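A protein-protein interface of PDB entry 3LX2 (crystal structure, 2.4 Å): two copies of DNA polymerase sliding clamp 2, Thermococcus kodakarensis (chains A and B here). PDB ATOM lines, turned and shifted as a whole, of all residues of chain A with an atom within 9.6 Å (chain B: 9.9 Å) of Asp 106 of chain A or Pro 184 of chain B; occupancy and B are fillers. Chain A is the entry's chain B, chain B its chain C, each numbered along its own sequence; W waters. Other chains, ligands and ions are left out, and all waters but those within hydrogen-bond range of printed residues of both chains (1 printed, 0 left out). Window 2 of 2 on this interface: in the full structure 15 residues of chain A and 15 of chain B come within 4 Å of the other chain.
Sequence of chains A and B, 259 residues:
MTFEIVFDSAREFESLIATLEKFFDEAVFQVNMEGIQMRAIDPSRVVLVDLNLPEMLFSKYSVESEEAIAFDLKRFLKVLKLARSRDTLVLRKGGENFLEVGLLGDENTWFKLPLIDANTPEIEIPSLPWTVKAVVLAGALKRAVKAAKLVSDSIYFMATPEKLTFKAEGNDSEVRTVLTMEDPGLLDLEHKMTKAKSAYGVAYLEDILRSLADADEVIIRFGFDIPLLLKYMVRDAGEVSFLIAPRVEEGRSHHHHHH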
ATOM      1  N   ALA A  83     -33.198   9.841 -11.139  1.00  0.00           N
ATOM      2  CA  ALA A  83     -33.659  11.043 -10.498  1.00  0.00           C
ATOM      3  C   ALA A  83     -33.191  11.041  -9.073  1.00  0.00           C
ATOM      4  O   ALA A  83     -33.258  10.031  -8.390  1.00  0.00           O
ATOM      5  CB  ALA A  83     -35.148  11.132 -10.561  1.00  0.00           C
ATOM      6  N   ARG A  84     -32.669  12.171  -8.643  1.00  0.00           N
ATOM      7  CA  ARG A  84     -32.177  12.333  -7.260  1.00  0.00           C
ATOM      8  C   ARG A  84     -33.303  12.798  -6.313  1.00  0.00           C
ATOM      9  O   ARG A  84     -34.389  13.184  -6.768  1.00  0.00           O
ATOM     10  CB  ARG A  84     -30.993  13.319  -7.224  1.00  0.00           C
ATOM     11  CG  ARG A  84     -29.709  12.686  -7.703  1.00  0.00           C
ATOM     12  CD  ARG A  84     -28.438  13.488  -7.352  1.00  0.00           C
ATOM     13  NE  ARG A  84     -28.129  13.592  -5.913  1.00  0.00           N
ATOM     14  CZ  ARG A  84     -27.755  12.594  -5.095  1.00  0.00           C
ATOM     15  NH1 ARG A  84     -27.647  11.327  -5.509  1.00  0.00           N
ATOM     16  NH2 ARG A  84     -27.503  12.870  -3.817  1.00  0.00           N
ATOM     17  N   SER A  85     -33.026  12.786  -5.011  1.00  0.00           N
ATOM     18  CA  SER A  85     -33.974  13.234  -3.986  1.00  0.00           C
ATOM     19  C   SER A  85     -34.943  14.362  -4.390  1.00  0.00           C
ATOM     20  O   SER A  85     -36.143  14.156  -4.409  1.00  0.00           O
ATOM     21  CB  SER A  85     -33.251  13.568  -2.663  1.00  0.00           C
ATOM     22  OG  SER A  85     -34.141  14.169  -1.712  1.00  0.00           O
ATOM     23  N   ARG A  86     -34.476  15.550  -4.702  1.00  0.00           N
ATOM     24  CA  ARG A  86     -35.460  16.586  -4.858  1.00  0.00           C
ATOM     25  C   ARG A  86     -35.796  16.976  -6.313  1.00  0.00           C
ATOM     26  O   ARG A  86     -36.545  17.954  -6.553  1.00  0.00           O
ATOM     27  CB  ARG A  86     -35.098  17.799  -3.976  1.00  0.00           C
ATOM     28  CG  ARG A  86     -35.390  17.580  -2.469  1.00  0.00           C
ATOM     29  CD  ARG A  86     -35.580  18.898  -1.641  1.00  0.00           C
ATOM     30  NE  ARG A  86     -36.127  18.603  -0.293  1.00  0.00           N
ATOM     31  CZ  ARG A  86     -37.425  18.435   0.022  1.00  0.00           C
ATOM     32  NH1 ARG A  86     -38.389  18.556  -0.898  1.00  0.00           N
ATOM     33  NH2 ARG A  86     -37.772  18.146   1.279  1.00  0.00           N
ATOM     34  N   ASP A  87     -35.286  16.205  -7.273  1.00  0.00           N
ATOM     35  CA  ASP A  87     -35.375  16.557  -8.691  1.00  0.00           C
ATOM     36  C   ASP A  87     -36.804  16.844  -9.187  1.00  0.00           C
ATOM     37  O   ASP A  87     -37.740  16.108  -8.901  1.00  0.00           O
ATOM     38  CB  ASP A  87     -34.686  15.489  -9.563  1.00  0.00           C
ATOM     39  CG  ASP A  87     -33.126  15.483  -9.425  1.00  0.00           C
ATOM     40  OD1 ASP A  87     -32.507  16.550  -9.181  1.00  0.00           O
ATOM     41  OD2 ASP A  87     -32.514  14.400  -9.595  1.00  0.00           O
ATOM     42  N   THR A  88     -36.953  17.952  -9.903  1.00  0.00           N
ATOM     43  CA  THR A  88     -38.135  18.244 -10.728  1.00  0.00           C
ATOM     44  C   THR A  88     -38.079  17.404 -12.014  1.00  0.00           C
ATOM     45  O   THR A  88     -37.004  17.010 -12.465  1.00  0.00           O
ATOM     46  CB  THR A  88     -38.168  19.745 -11.092  1.00  0.00           C
ATOM     47  OG1 THR A  88     -37.994  20.526  -9.901  1.00  0.00           O
ATOM     48  CG2 THR A  88     -39.489  20.167 -11.738  1.00  0.00           C
ATOM     49  N   LEU A 103     -34.562  16.192 -15.909  1.00  0.00           N
ATOM     50  CA  LEU A 103     -34.433  15.982 -14.466  1.00  0.00           C
ATOM     51  C   LEU A 103     -33.702  17.182 -13.841  1.00  0.00           C
ATOM     52  O   LEU A 103     -32.475  17.268 -13.900  1.00  0.00           O
ATOM     53  CB  LEU A 103     -33.694  14.651 -14.196  1.00  0.00           C
ATOM     54  CG  LEU A 103     -34.378  13.372 -14.744  1.00  0.00           C
ATOM     55  CD1 LEU A 103     -33.631  12.130 -14.400  1.00  0.00           C
ATOM     56  CD2 LEU A 103     -35.816  13.249 -14.268  1.00  0.00           C
ATOM     57  N   LEU A 104     -34.457  18.114 -13.255  1.00  0.00           N
ATOM     58  CA  LEU A 104     -33.885  19.411 -12.871  1.00  0.00           C
ATOM     59  C   LEU A 104     -33.571  19.540 -11.382  1.00  0.00           C
ATOM     60  O   LEU A 104     -34.472  19.446 -10.521  1.00  0.00           O
ATOM     61  CB  LEU A 104     -34.746  20.575 -13.344  1.00  0.00           C
ATOM     62  CG  LEU A 104     -35.163  20.647 -14.806  1.00  0.00           C
ATOM     63  CD1 LEU A 104     -35.686  22.025 -15.083  1.00  0.00           C
ATOM     64  CD2 LEU A 104     -34.030  20.341 -15.727  1.00  0.00           C
ATOM     65  N   GLY A 105     -32.293  19.761 -11.083  1.00  0.00           N
ATOM     66  CA  GLY A 105     -31.837  19.745  -9.691  1.00  0.00           C
ATOM     67  C   GLY A 105     -30.456  20.308  -9.436  1.00  0.00           C
ATOM     68  O   GLY A 105     -30.125  21.343  -9.966  1.00  0.00           O
ATOM     69  N   ASP A 106     -29.677  19.651  -8.577  1.00  0.00           N
ATOM     70  CA  ASP A 106     -28.244  19.962  -8.421  1.00  0.00           C
ATOM     71  C   ASP A 106     -27.517  19.956  -9.791  1.00  0.00           C
ATOM     72  O   ASP A 106     -26.680  20.833 -10.084  1.00  0.00           O
ATOM     73  CB  ASP A 106     -27.596  18.949  -7.486  1.00  0.00           C
ATOM     74  CG  ASP A 106     -27.788  19.300  -6.004  1.00  0.00           C
ATOM     75  OD1 ASP A 106     -28.531  20.279  -5.675  1.00  0.00           O
ATOM     76  OD2 ASP A 106     -27.156  18.592  -5.171  1.00  0.00           O
ATOM     77  N   GLU A 107     -27.856  18.930 -10.592  1.00  0.00           N
ATOM     78  CA  GLU A 107     -27.486  18.787 -11.997  1.00  0.00           C
ATOM     79  C   GLU A 107     -28.752  18.965 -12.828  1.00  0.00           C
ATOM     80  O   GLU A 107     -29.839  18.681 -12.358  1.00  0.00           O
ATOM     81  CB  GLU A 107     -26.885  17.394 -12.220  1.00  0.00           C
ATOM     82  CG  GLU A 107     -25.714  17.039 -11.226  1.00  0.00           C
ATOM     83  CD  GLU A 107     -26.084  16.056 -10.059  1.00  0.00           C
ATOM     84  OE1 GLU A 107     -27.070  15.256 -10.141  1.00  0.00           O
ATOM     85  OE2 GLU A 107     -25.342  16.073  -9.047  1.00  0.00           O
ATOM     86  N   ASN A 108     -28.638  19.496 -14.034  1.00  0.00           N
ATOM     87  CA  ASN A 108     -29.765  19.496 -14.945  1.00  0.00           C
ATOM     88  C   ASN A 108     -29.460  18.427 -15.968  1.00  0.00           C
ATOM     89  O   ASN A 108     -28.362  18.404 -16.518  1.00  0.00           O
ATOM     90  CB  ASN A 108     -29.946  20.850 -15.605  1.00  0.00           C
ATOM     91  CG  ASN A 108     -30.672  21.846 -14.712  1.00  0.00           C
ATOM     92  OD1 ASN A 108     -30.877  21.607 -13.524  1.00  0.00           O
ATOM     93  ND2 ASN A 108     -31.076  22.970 -15.289  1.00  0.00           N
ATOM     94  N   THR A 109     -30.390  17.500 -16.180  1.00  0.00           N
ATOM     95  CA  THR A 109     -30.182  16.489 -17.210  1.00  0.00           C
ATOM     96  C   THR A 109     -31.352  16.381 -18.146  1.00  0.00           C
ATOM     97  O   THR A 109     -32.485  16.272 -17.699  1.00  0.00           O
ATOM     98  CB  THR A 109     -29.893  15.132 -16.629  1.00  0.00           C
ATOM     99  OG1 THR A 109     -28.773  15.240 -15.741  1.00  0.00           O
ATOM    100  CG2 THR A 109     -29.573  14.164 -17.742  1.00  0.00           C
ATOM    101  N   VAL B 135     -12.591  21.627 -11.066  1.00  0.00           N
ATOM    102  CA  VAL B 135     -12.808  20.867  -9.828  1.00  0.00           C
ATOM    103  C   VAL B 135     -14.315  20.632  -9.732  1.00  0.00           C
ATOM    104  O   VAL B 135     -15.125  21.554  -9.887  1.00  0.00           O
ATOM    105  CB  VAL B 135     -12.260  21.573  -8.575  1.00  0.00           C
ATOM    106  CG1 VAL B 135     -12.460  20.723  -7.308  1.00  0.00           C
ATOM    107  CG2 VAL B 135     -10.706  21.936  -8.760  1.00  0.00           C
ATOM    108  N   VAL B 136     -14.692  19.376  -9.562  1.00  0.00           N
ATOM    109  CA  VAL B 136     -16.072  19.024  -9.566  1.00  0.00           C
ATOM    110  C   VAL B 136     -16.343  17.967  -8.494  1.00  0.00           C
ATOM    111  O   VAL B 136     -15.413  17.322  -7.992  1.00  0.00           O
ATOM    112  CB  VAL B 136     -16.464  18.464 -10.941  1.00  0.00           C
ATOM    113  CG1 VAL B 136     -16.608  19.585 -11.991  1.00  0.00           C
ATOM    114  CG2 VAL B 136     -15.413  17.480 -11.364  1.00  0.00           C
ATOM    115  N   LEU B 137     -17.606  17.767  -8.143  1.00  0.00           N
ATOM    116  CA  LEU B 137     -17.906  16.720  -7.138  1.00  0.00           C
ATOM    117  C   LEU B 137     -18.047  15.384  -7.819  1.00  0.00           C
ATOM    118  O   LEU B 137     -18.717  15.261  -8.834  1.00  0.00           O
ATOM    119  CB  LEU B 137     -19.138  17.058  -6.272  1.00  0.00           C
ATOM    120  CG  LEU B 137     -19.015  18.263  -5.331  1.00  0.00           C
ATOM    121  CD1 LEU B 137     -20.225  18.320  -4.377  1.00  0.00           C
ATOM    122  CD2 LEU B 137     -17.735  18.301  -4.471  1.00  0.00           C
ATOM    123  N   ALA B 138     -17.412  14.367  -7.289  1.00  0.00           N
ATOM    124  CA  ALA B 138     -17.623  13.038  -7.902  1.00  0.00           C
ATOM    125  C   ALA B 138     -19.104  12.719  -8.200  1.00  0.00           C
ATOM    126  O   ALA B 138     -19.436  12.119  -9.220  1.00  0.00           O
ATOM    127  CB  ALA B 138     -17.041  12.006  -7.053  1.00  0.00           C
ATOM    128  N   GLY B 139     -20.004  13.132  -7.326  1.00  0.00           N
ATOM    129  CA  GLY B 139     -21.396  12.757  -7.470  1.00  0.00           C
ATOM    130  C   GLY B 139     -21.927  13.241  -8.786  1.00  0.00           C
ATOM    131  O   GLY B 139     -22.571  12.498  -9.542  1.00  0.00           O
ATOM    132  N   ALA B 140     -21.644  14.506  -9.051  1.00  0.00           N
ATOM    133  CA  ALA B 140     -21.994  15.142 -10.298  1.00  0.00           C
ATOM    134  C   ALA B 140     -21.500  14.361 -11.525  1.00  0.00           C
ATOM    135  O   ALA B 140     -22.272  14.190 -12.496  1.00  0.00           O
ATOM    136  CB  ALA B 140     -21.457  16.595 -10.323  1.00  0.00           C
ATOM    137  N   LEU B 141     -20.234  13.915 -11.503  1.00  0.00           N
ATOM    138  CA  LEU B 141     -19.697  13.232 -12.668  1.00  0.00           C
ATOM    139  C   LEU B 141     -20.361  11.883 -12.787  1.00  0.00           C
ATOM    140  O   LEU B 141     -20.434  11.322 -13.872  1.00  0.00           O
ATOM    141  CB  LEU B 141     -18.185  12.995 -12.589  1.00  0.00           C
ATOM    142  CG  LEU B 141     -17.138  14.093 -12.754  1.00  0.00           C
ATOM    143  CD1 LEU B 141     -15.751  13.491 -12.701  1.00  0.00           C
ATOM    144  CD2 LEU B 141     -17.337  14.861 -14.058  1.00  0.00           C
ATOM    145  N   ARG B 143     -23.450  11.078 -12.004  1.00  0.00           N
ATOM    146  CA  ARG B 143     -24.647  11.360 -12.723  1.00  0.00           C
ATOM    147  C   ARG B 143     -24.255  11.376 -14.167  1.00  0.00           C
ATOM    148  O   ARG B 143     -24.736  10.549 -14.942  1.00  0.00           O
ATOM    149  CB  ARG B 143     -25.235  12.722 -12.327  1.00  0.00           C
ATOM    150  CG  ARG B 143     -26.211  13.336 -13.343  1.00  0.00           C
ATOM    151  CD  ARG B 143     -27.411  12.435 -13.644  1.00  0.00           C
ATOM    152  NE  ARG B 143     -28.420  12.443 -12.571  1.00  0.00           N
ATOM    153  CZ  ARG B 143     -29.395  13.347 -12.461  1.00  0.00           C
ATOM    154  NH1 ARG B 143     -29.496  14.357 -13.340  1.00  0.00           N
ATOM    155  NH2 ARG B 143     -30.251  13.254 -11.457  1.00  0.00           N
ATOM    156  N   LEU B 164     -19.897  23.265 -17.930  1.00  0.00           N
ATOM    157  CA  LEU B 164     -19.409  21.965 -18.337  1.00  0.00           C
ATOM    158  C   LEU B 164     -20.566  21.144 -18.831  1.00  0.00           C
ATOM    159  O   LEU B 164     -21.570  21.009 -18.119  1.00  0.00           O
ATOM    160  CB  LEU B 164     -18.698  21.200 -17.228  1.00  0.00           C
ATOM    161  CG  LEU B 164     -17.311  21.642 -16.788  1.00  0.00           C
ATOM    162  CD1 LEU B 164     -16.850  20.815 -15.627  1.00  0.00           C
ATOM    163  CD2 LEU B 164     -16.311  21.553 -17.941  1.00  0.00           C
ATOM    164  N   THR B 177     -25.876  16.598 -19.695  1.00  0.00           N
ATOM    165  CA  THR B 177     -25.846  17.044 -18.324  1.00  0.00           C
ATOM    166  C   THR B 177     -24.980  18.311 -18.290  1.00  0.00           C
ATOM    167  O   THR B 177     -23.834  18.342 -18.744  1.00  0.00           O
ATOM    168  CB  THR B 177     -25.239  15.976 -17.382  1.00  0.00           C
ATOM    169  OG1 THR B 177     -25.984  14.743 -17.452  1.00  0.00           O
ATOM    170  CG2 THR B 177     -25.205  16.483 -15.962  1.00  0.00           C
ATOM    171  N   VAL B 178     -25.543  19.349 -17.719  1.00  0.00           N
ATOM    172  CA  VAL B 178     -24.950  20.644 -17.740  1.00  0.00           C
ATOM    173  C   VAL B 178     -24.618  21.076 -16.321  1.00  0.00           C
ATOM    174  O   VAL B 178     -25.388  20.896 -15.394  1.00  0.00           O
ATOM    175  CB  VAL B 178     -25.884  21.609 -18.464  1.00  0.00           C
ATOM    176  CG1 VAL B 178     -25.650  23.063 -18.062  1.00  0.00           C
ATOM    177  CG2 VAL B 178     -25.676  21.437 -19.945  1.00  0.00           C
ATOM    178  N   LEU B 179     -23.449  21.649 -16.156  1.00  0.00           N
ATOM    179  CA  LEU B 179     -23.010  22.024 -14.848  1.00  0.00           C
ATOM    180  C   LEU B 179     -22.442  23.441 -14.947  1.00  0.00           C
ATOM    181  O   LEU B 179     -21.433  23.676 -15.632  1.00  0.00           O
ATOM    182  CB  LEU B 179     -21.996  20.980 -14.391  1.00  0.00           C
ATOM    183  CG  LEU B 179     -21.710  20.655 -12.933  1.00  0.00           C
ATOM    184  CD1 LEU B 179     -22.956  20.097 -12.154  1.00  0.00           C
ATOM    185  CD2 LEU B 179     -20.557  19.647 -12.940  1.00  0.00           C
ATOM    186  N   THR B 180     -23.144  24.388 -14.326  1.00  0.00           N
ATOM    187  CA  THR B 180     -22.703  25.791 -14.266  1.00  0.00           C
ATOM    188  C   THR B 180     -22.124  26.084 -12.909  1.00  0.00           C
ATOM    189  O   THR B 180     -22.291  25.317 -11.982  1.00  0.00           O
ATOM    190  CB  THR B 180     -23.874  26.775 -14.426  1.00  0.00           C
ATOM    191  OG1 THR B 180     -24.610  26.862 -13.180  1.00  0.00           O
ATOM    192  CG2 THR B 180     -24.797  26.344 -15.566  1.00  0.00           C
ATOM    193  N   MET B 181     -21.521  27.255 -12.792  1.00  0.00           N
ATOM    194  CA  MET B 181     -20.906  27.727 -11.558  1.00  0.00           C
ATOM    195  C   MET B 181     -21.863  28.001 -10.391  1.00  0.00           C
ATOM    196  O   MET B 181     -21.446  27.989  -9.197  1.00  0.00           O
ATOM    197  CB  MET B 181     -20.106  28.982 -11.854  1.00  0.00           C
ATOM    198  CG  MET B 181     -18.980  29.158 -10.892  1.00  0.00           C
ATOM    199  SD  MET B 181     -17.516  28.329 -11.513  1.00  0.00           S
ATOM    200  CE  MET B 181     -16.905  27.682  -9.971  1.00  0.00           C
ATOM    201  N   GLU B 182     -23.126  28.262 -10.730  1.00  0.00           N
ATOM    202  CA  GLU B 182     -24.218  28.331  -9.762  1.00  0.00           C
ATOM    203  C   GLU B 182     -24.410  26.952  -9.081  1.00  0.00           C
ATOM    204  O   GLU B 182     -24.912  26.872  -7.959  1.00  0.00           O
ATOM    205  CB  GLU B 182     -25.523  28.755 -10.465  1.00  0.00           C
ATOM    206  CG  GLU B 182     -25.564  30.190 -11.121  1.00  0.00           C
ATOM    207  CD  GLU B 182     -24.418  30.495 -12.146  1.00  0.00           C
ATOM    208  OE1 GLU B 182     -24.384  29.911 -13.279  1.00  0.00           O
ATOM    209  OE2 GLU B 182     -23.558  31.352 -11.800  1.00  0.00           O
ATOM    210  N   ASP B 183     -23.982  25.874  -9.738  1.00  0.00           N
ATOM    211  CA  ASP B 183     -24.288  24.501  -9.266  1.00  0.00           C
ATOM    212  C   ASP B 183     -23.303  24.061  -8.211  1.00  0.00           C
ATOM    213  O   ASP B 183     -22.131  24.381  -8.322  1.00  0.00           O
ATOM    214  CB  ASP B 183     -24.343  23.521 -10.438  1.00  0.00           C
ATOM    215  CG  ASP B 183     -25.431  23.898 -11.435  1.00  0.00           C
ATOM    216  OD1 ASP B 183     -26.351  24.560 -10.954  1.00  0.00           O
ATOM    217  OD2 ASP B 183     -25.401  23.569 -12.659  1.00  0.00           O
ATOM    218  N   PRO B 184     -23.780  23.350  -7.168  1.00  0.00           N
ATOM    219  CA  PRO B 184     -22.861  22.983  -6.097  1.00  0.00           C
ATOM    220  C   PRO B 184     -21.799  22.023  -6.579  1.00  0.00           C
ATOM    221  O   PRO B 184     -20.737  21.970  -5.996  1.00  0.00           O
ATOM    222  CB  PRO B 184     -23.767  22.281  -5.072  1.00  0.00           C
ATOM    223  CG  PRO B 184     -24.947  21.810  -5.845  1.00  0.00           C
ATOM    224  CD  PRO B 184     -25.158  22.903  -6.873  1.00  0.00           C
ATOM    225  N   GLY B 185     -22.079  21.269  -7.628  1.00  0.00           N
ATOM    226  CA  GLY B 185     -21.159  20.252  -8.079  1.00  0.00           C
ATOM    227  C   GLY B 185     -19.919  20.713  -8.824  1.00  0.00           C
ATOM    228  O   GLY B 185     -19.047  19.901  -9.124  1.00  0.00           O
ATOM    229  N   LEU B 186     -19.831  21.999  -9.114  1.00  0.00           N
ATOM    230  CA  LEU B 186     -18.703  22.562  -9.836  1.00  0.00           C
ATOM    231  C   LEU B 186     -18.036  23.626  -8.979  1.00  0.00           C
ATOM    232  O   LEU B 186     -18.626  24.666  -8.754  1.00  0.00           O
ATOM    233  CB  LEU B 186     -19.205  23.173 -11.153  1.00  0.00           C
ATOM    234  CG  LEU B 186     -18.264  24.021 -12.014  1.00  0.00           C
ATOM    235  CD1 LEU B 186     -16.979  23.227 -12.337  1.00  0.00           C
ATOM    236  CD2 LEU B 186     -18.951  24.574 -13.287  1.00  0.00           C
ATOM    237  N   LEU B 187     -16.820  23.372  -8.498  1.00  0.00           N
ATOM    238  CA  LEU B 187     -16.143  24.296  -7.592  1.00  0.00           C
ATOM    239  C   LEU B 187     -15.224  25.349  -8.255  1.00  0.00           C
ATOM    240  O   LEU B 187     -14.930  26.447  -7.698  1.00  0.00           O
ATOM    241  CB  LEU B 187     -15.305  23.503  -6.589  1.00  0.00           C
ATOM    242  CG  LEU B 187     -15.970  22.441  -5.708  1.00  0.00           C
ATOM    243  CD1 LEU B 187     -15.193  22.313  -4.360  1.00  0.00           C
ATOM    244  CD2 LEU B 187     -17.460  22.715  -5.439  1.00  0.00           C
ATOM    245  N   ASP B 188     -14.726  25.007  -9.431  1.00  0.00           N
ATOM    246  CA  ASP B 188     -13.583  25.695  -9.945  1.00  0.00           C
ATOM    247  C   ASP B 188     -13.513  25.439 -11.427  1.00  0.00           C
ATOM    248  O   ASP B 188     -13.608  24.305 -11.876  1.00  0.00           O
ATOM    249  CB  ASP B 188     -12.340  25.166  -9.230  1.00  0.00           C
ATOM    250  CG  ASP B 188     -11.058  25.781  -9.749  1.00  0.00           C
ATOM    251  OD1 ASP B 188     -10.583  26.763  -9.129  1.00  0.00           O
ATOM    252  OD2 ASP B 188     -10.531  25.309 -10.788  1.00  0.00           O
ATOM    253  N   ASP B 214     -19.877  10.753  -3.330  1.00  0.00           N
ATOM    254  CA  ASP B 214     -20.491  11.880  -4.030  1.00  0.00           C
ATOM    255  C   ASP B 214     -19.870  13.225  -3.690  1.00  0.00           C
ATOM    256  O   ASP B 214     -19.761  14.093  -4.552  1.00  0.00           O
ATOM    257  CB  ASP B 214     -21.988  11.947  -3.798  1.00  0.00           C
ATOM    258  CG  ASP B 214     -22.741  10.782  -4.434  1.00  0.00           C
ATOM    259  OD1 ASP B 214     -22.117   9.903  -5.106  1.00  0.00           O
ATOM    260  OD2 ASP B 214     -23.980  10.743  -4.237  1.00  0.00           O
ATOM    261  N   ALA B 215     -19.443  13.391  -2.452  1.00  0.00           N
ATOM    262  CA  ALA B 215     -18.878  14.663  -2.013  1.00  0.00           C
ATOM    263  C   ALA B 215     -17.373  14.831  -2.235  1.00  0.00           C
ATOM    264  O   ALA B 215     -16.815  15.874  -1.936  1.00  0.00           O
ATOM    265  CB  ALA B 215     -19.245  14.922  -0.540  1.00  0.00           C
ATOM    266  N   ASP B 216     -16.697  13.810  -2.741  1.00  0.00           N
ATOM    267  CA  ASP B 216     -15.264  13.955  -3.069  1.00  0.00           C
ATOM    268  C   ASP B 216     -14.967  14.912  -4.224  1.00  0.00           C
ATOM    269  O   ASP B 216     -15.649  14.942  -5.249  1.00  0.00           O
ATOM    270  CB  ASP B 216     -14.643  12.603  -3.349  1.00  0.00           C
ATOM    271  CG  ASP B 216     -14.568  11.736  -2.116  1.00  0.00           C
ATOM    272  OD1 ASP B 216     -14.279  12.275  -1.009  1.00  0.00           O
ATOM    273  OD2 ASP B 216     -14.806  10.523  -2.261  1.00  0.00           O
ATOM    274  N   GLU B 217     -13.938  15.714  -4.024  1.00  0.00           N
ATOM    275  CA  GLU B 217     -13.456  16.585  -5.065  1.00  0.00           C
ATOM    276  C   GLU B 217     -12.608  15.793  -6.055  1.00  0.00           C
ATOM    277  O   GLU B 217     -11.656  15.112  -5.662  1.00  0.00           O
ATOM    278  CB  GLU B 217     -12.620  17.677  -4.472  1.00  0.00           C
ATOM    279  CG  GLU B 217     -13.401  18.611  -3.628  1.00  0.00           C
ATOM    280  CD  GLU B 217     -12.555  19.761  -3.241  1.00  0.00           C
ATOM    281  OE1 GLU B 217     -11.403  19.784  -3.709  1.00  0.00           O
ATOM    282  OE2 GLU B 217     -13.018  20.629  -2.481  1.00  0.00           O
HETATM  283  O   HOH W   1     -24.232  20.212  -9.149  1.00  0.00           O
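Hydrophobic or aromatic side chains of chain B that line the printed part of chain A: Pro 184.
Glu 107 of chain A touches just these residues of chain B: Ala 140 and Arg 143.
Of the printed residues of chain B, Arg 84 of chain A touches Arg 143 (3.8 Å) and Asp 214 (3.9 Å).
Of the printed residues of chain B, Thr 109 of chain A touches Arg 143 and Thr 177.
Of the printed residues of chain A, Ala 140 of chain B touches Glu 107.
Printed residues of chain A within 4 Å of Arg 143 of chain B: Arg 84 (3.8 Å), Asp 87 (3.1 Å), Glu 107 (3.8 Å) and Thr 109 (2.7 Å).
Printed residues of chain A within 4 Å of Val 178 of chain B: Asn 108.
Thr 88 of chain A touches none of the printed residues of chain B.
The backbone NH (N) of Arg 84 of chain A sits at hydrogen-bond distance from the side-chain carboxylate (OD2) of Asp 87 of chain A, at 2.4 Å.
N of Leu 103 of chain A sits at hydrogen-bond distance from O of Thr 109 of chain A (2.7 Å).
The backbone NH (N) of Gly 105 of chain A sits at hydrogen-bond distance from the side-chain amide oxygen (OD1) of Asn 108 of chain A, 3.4 Å away.
The backbone NH (N) of Gly 139 of chain B lies within hydrogen-bond range of the backbone carbonyl oxygen (O) of Asp 214 of chain B (2.9 Å).
The backbone NH (N) of Thr 180 of chain B is in hydrogen-bond range of the side-chain carboxylate (OD2) of Asp 183 of chain B, at 2.9 Å.
No position is printed for both chains.
Of the 11 pairs that touch across the chains among the printed residues, none has its exchanged pair printed and touching as well.
Among the printed residues, pairs that only touch across the chains: Arg 84 of chain A with Arg 143 of chain B (3.8 Å), Asp 106 of chain A with Asp 183 of chain B (3.6 Å), Asp 106 of chain A with Pro 184 of chain B (3.8 Å), Glu 107 of chain A with Ala 140 of chain B (3.7 Å) and Asn 108 of chain A with Thr 177 of chain B (3.4 Å).
NH1 of Arg 84 of chain A is in salt-bridge range of OD2 of Asp 214 of chain B (3.9 Å).
OD2 of Asp 87 of chain A lies within salt-bridge range of NH2 of Arg 143 of chain B.
OE1 of Glu 107 of chain A is in salt-bridge range of NE of Arg 143 of chain B (3.95 Å).
N of Val 178 of chain B sits at hydrogen-bond distance from O of Asn 108 of chain A, 3.2 Å away.
The side-chain hydroxyl (OG1) of Thr 109 of chain A is in hydrogen-bond range of the guanidinium group (NH1) of Arg 143 of chain B (2.7 Å).
OG1 of Thr 109 of chain A sits at hydrogen-bond distance from OG1 of Thr 177 of chain B, 3.3 Å away.
Water W1 lies within hydrogen-bond range of O of Asp 106 of chain A (2.7 Å) and N of Gly 185 of chain B (2.8 Å).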
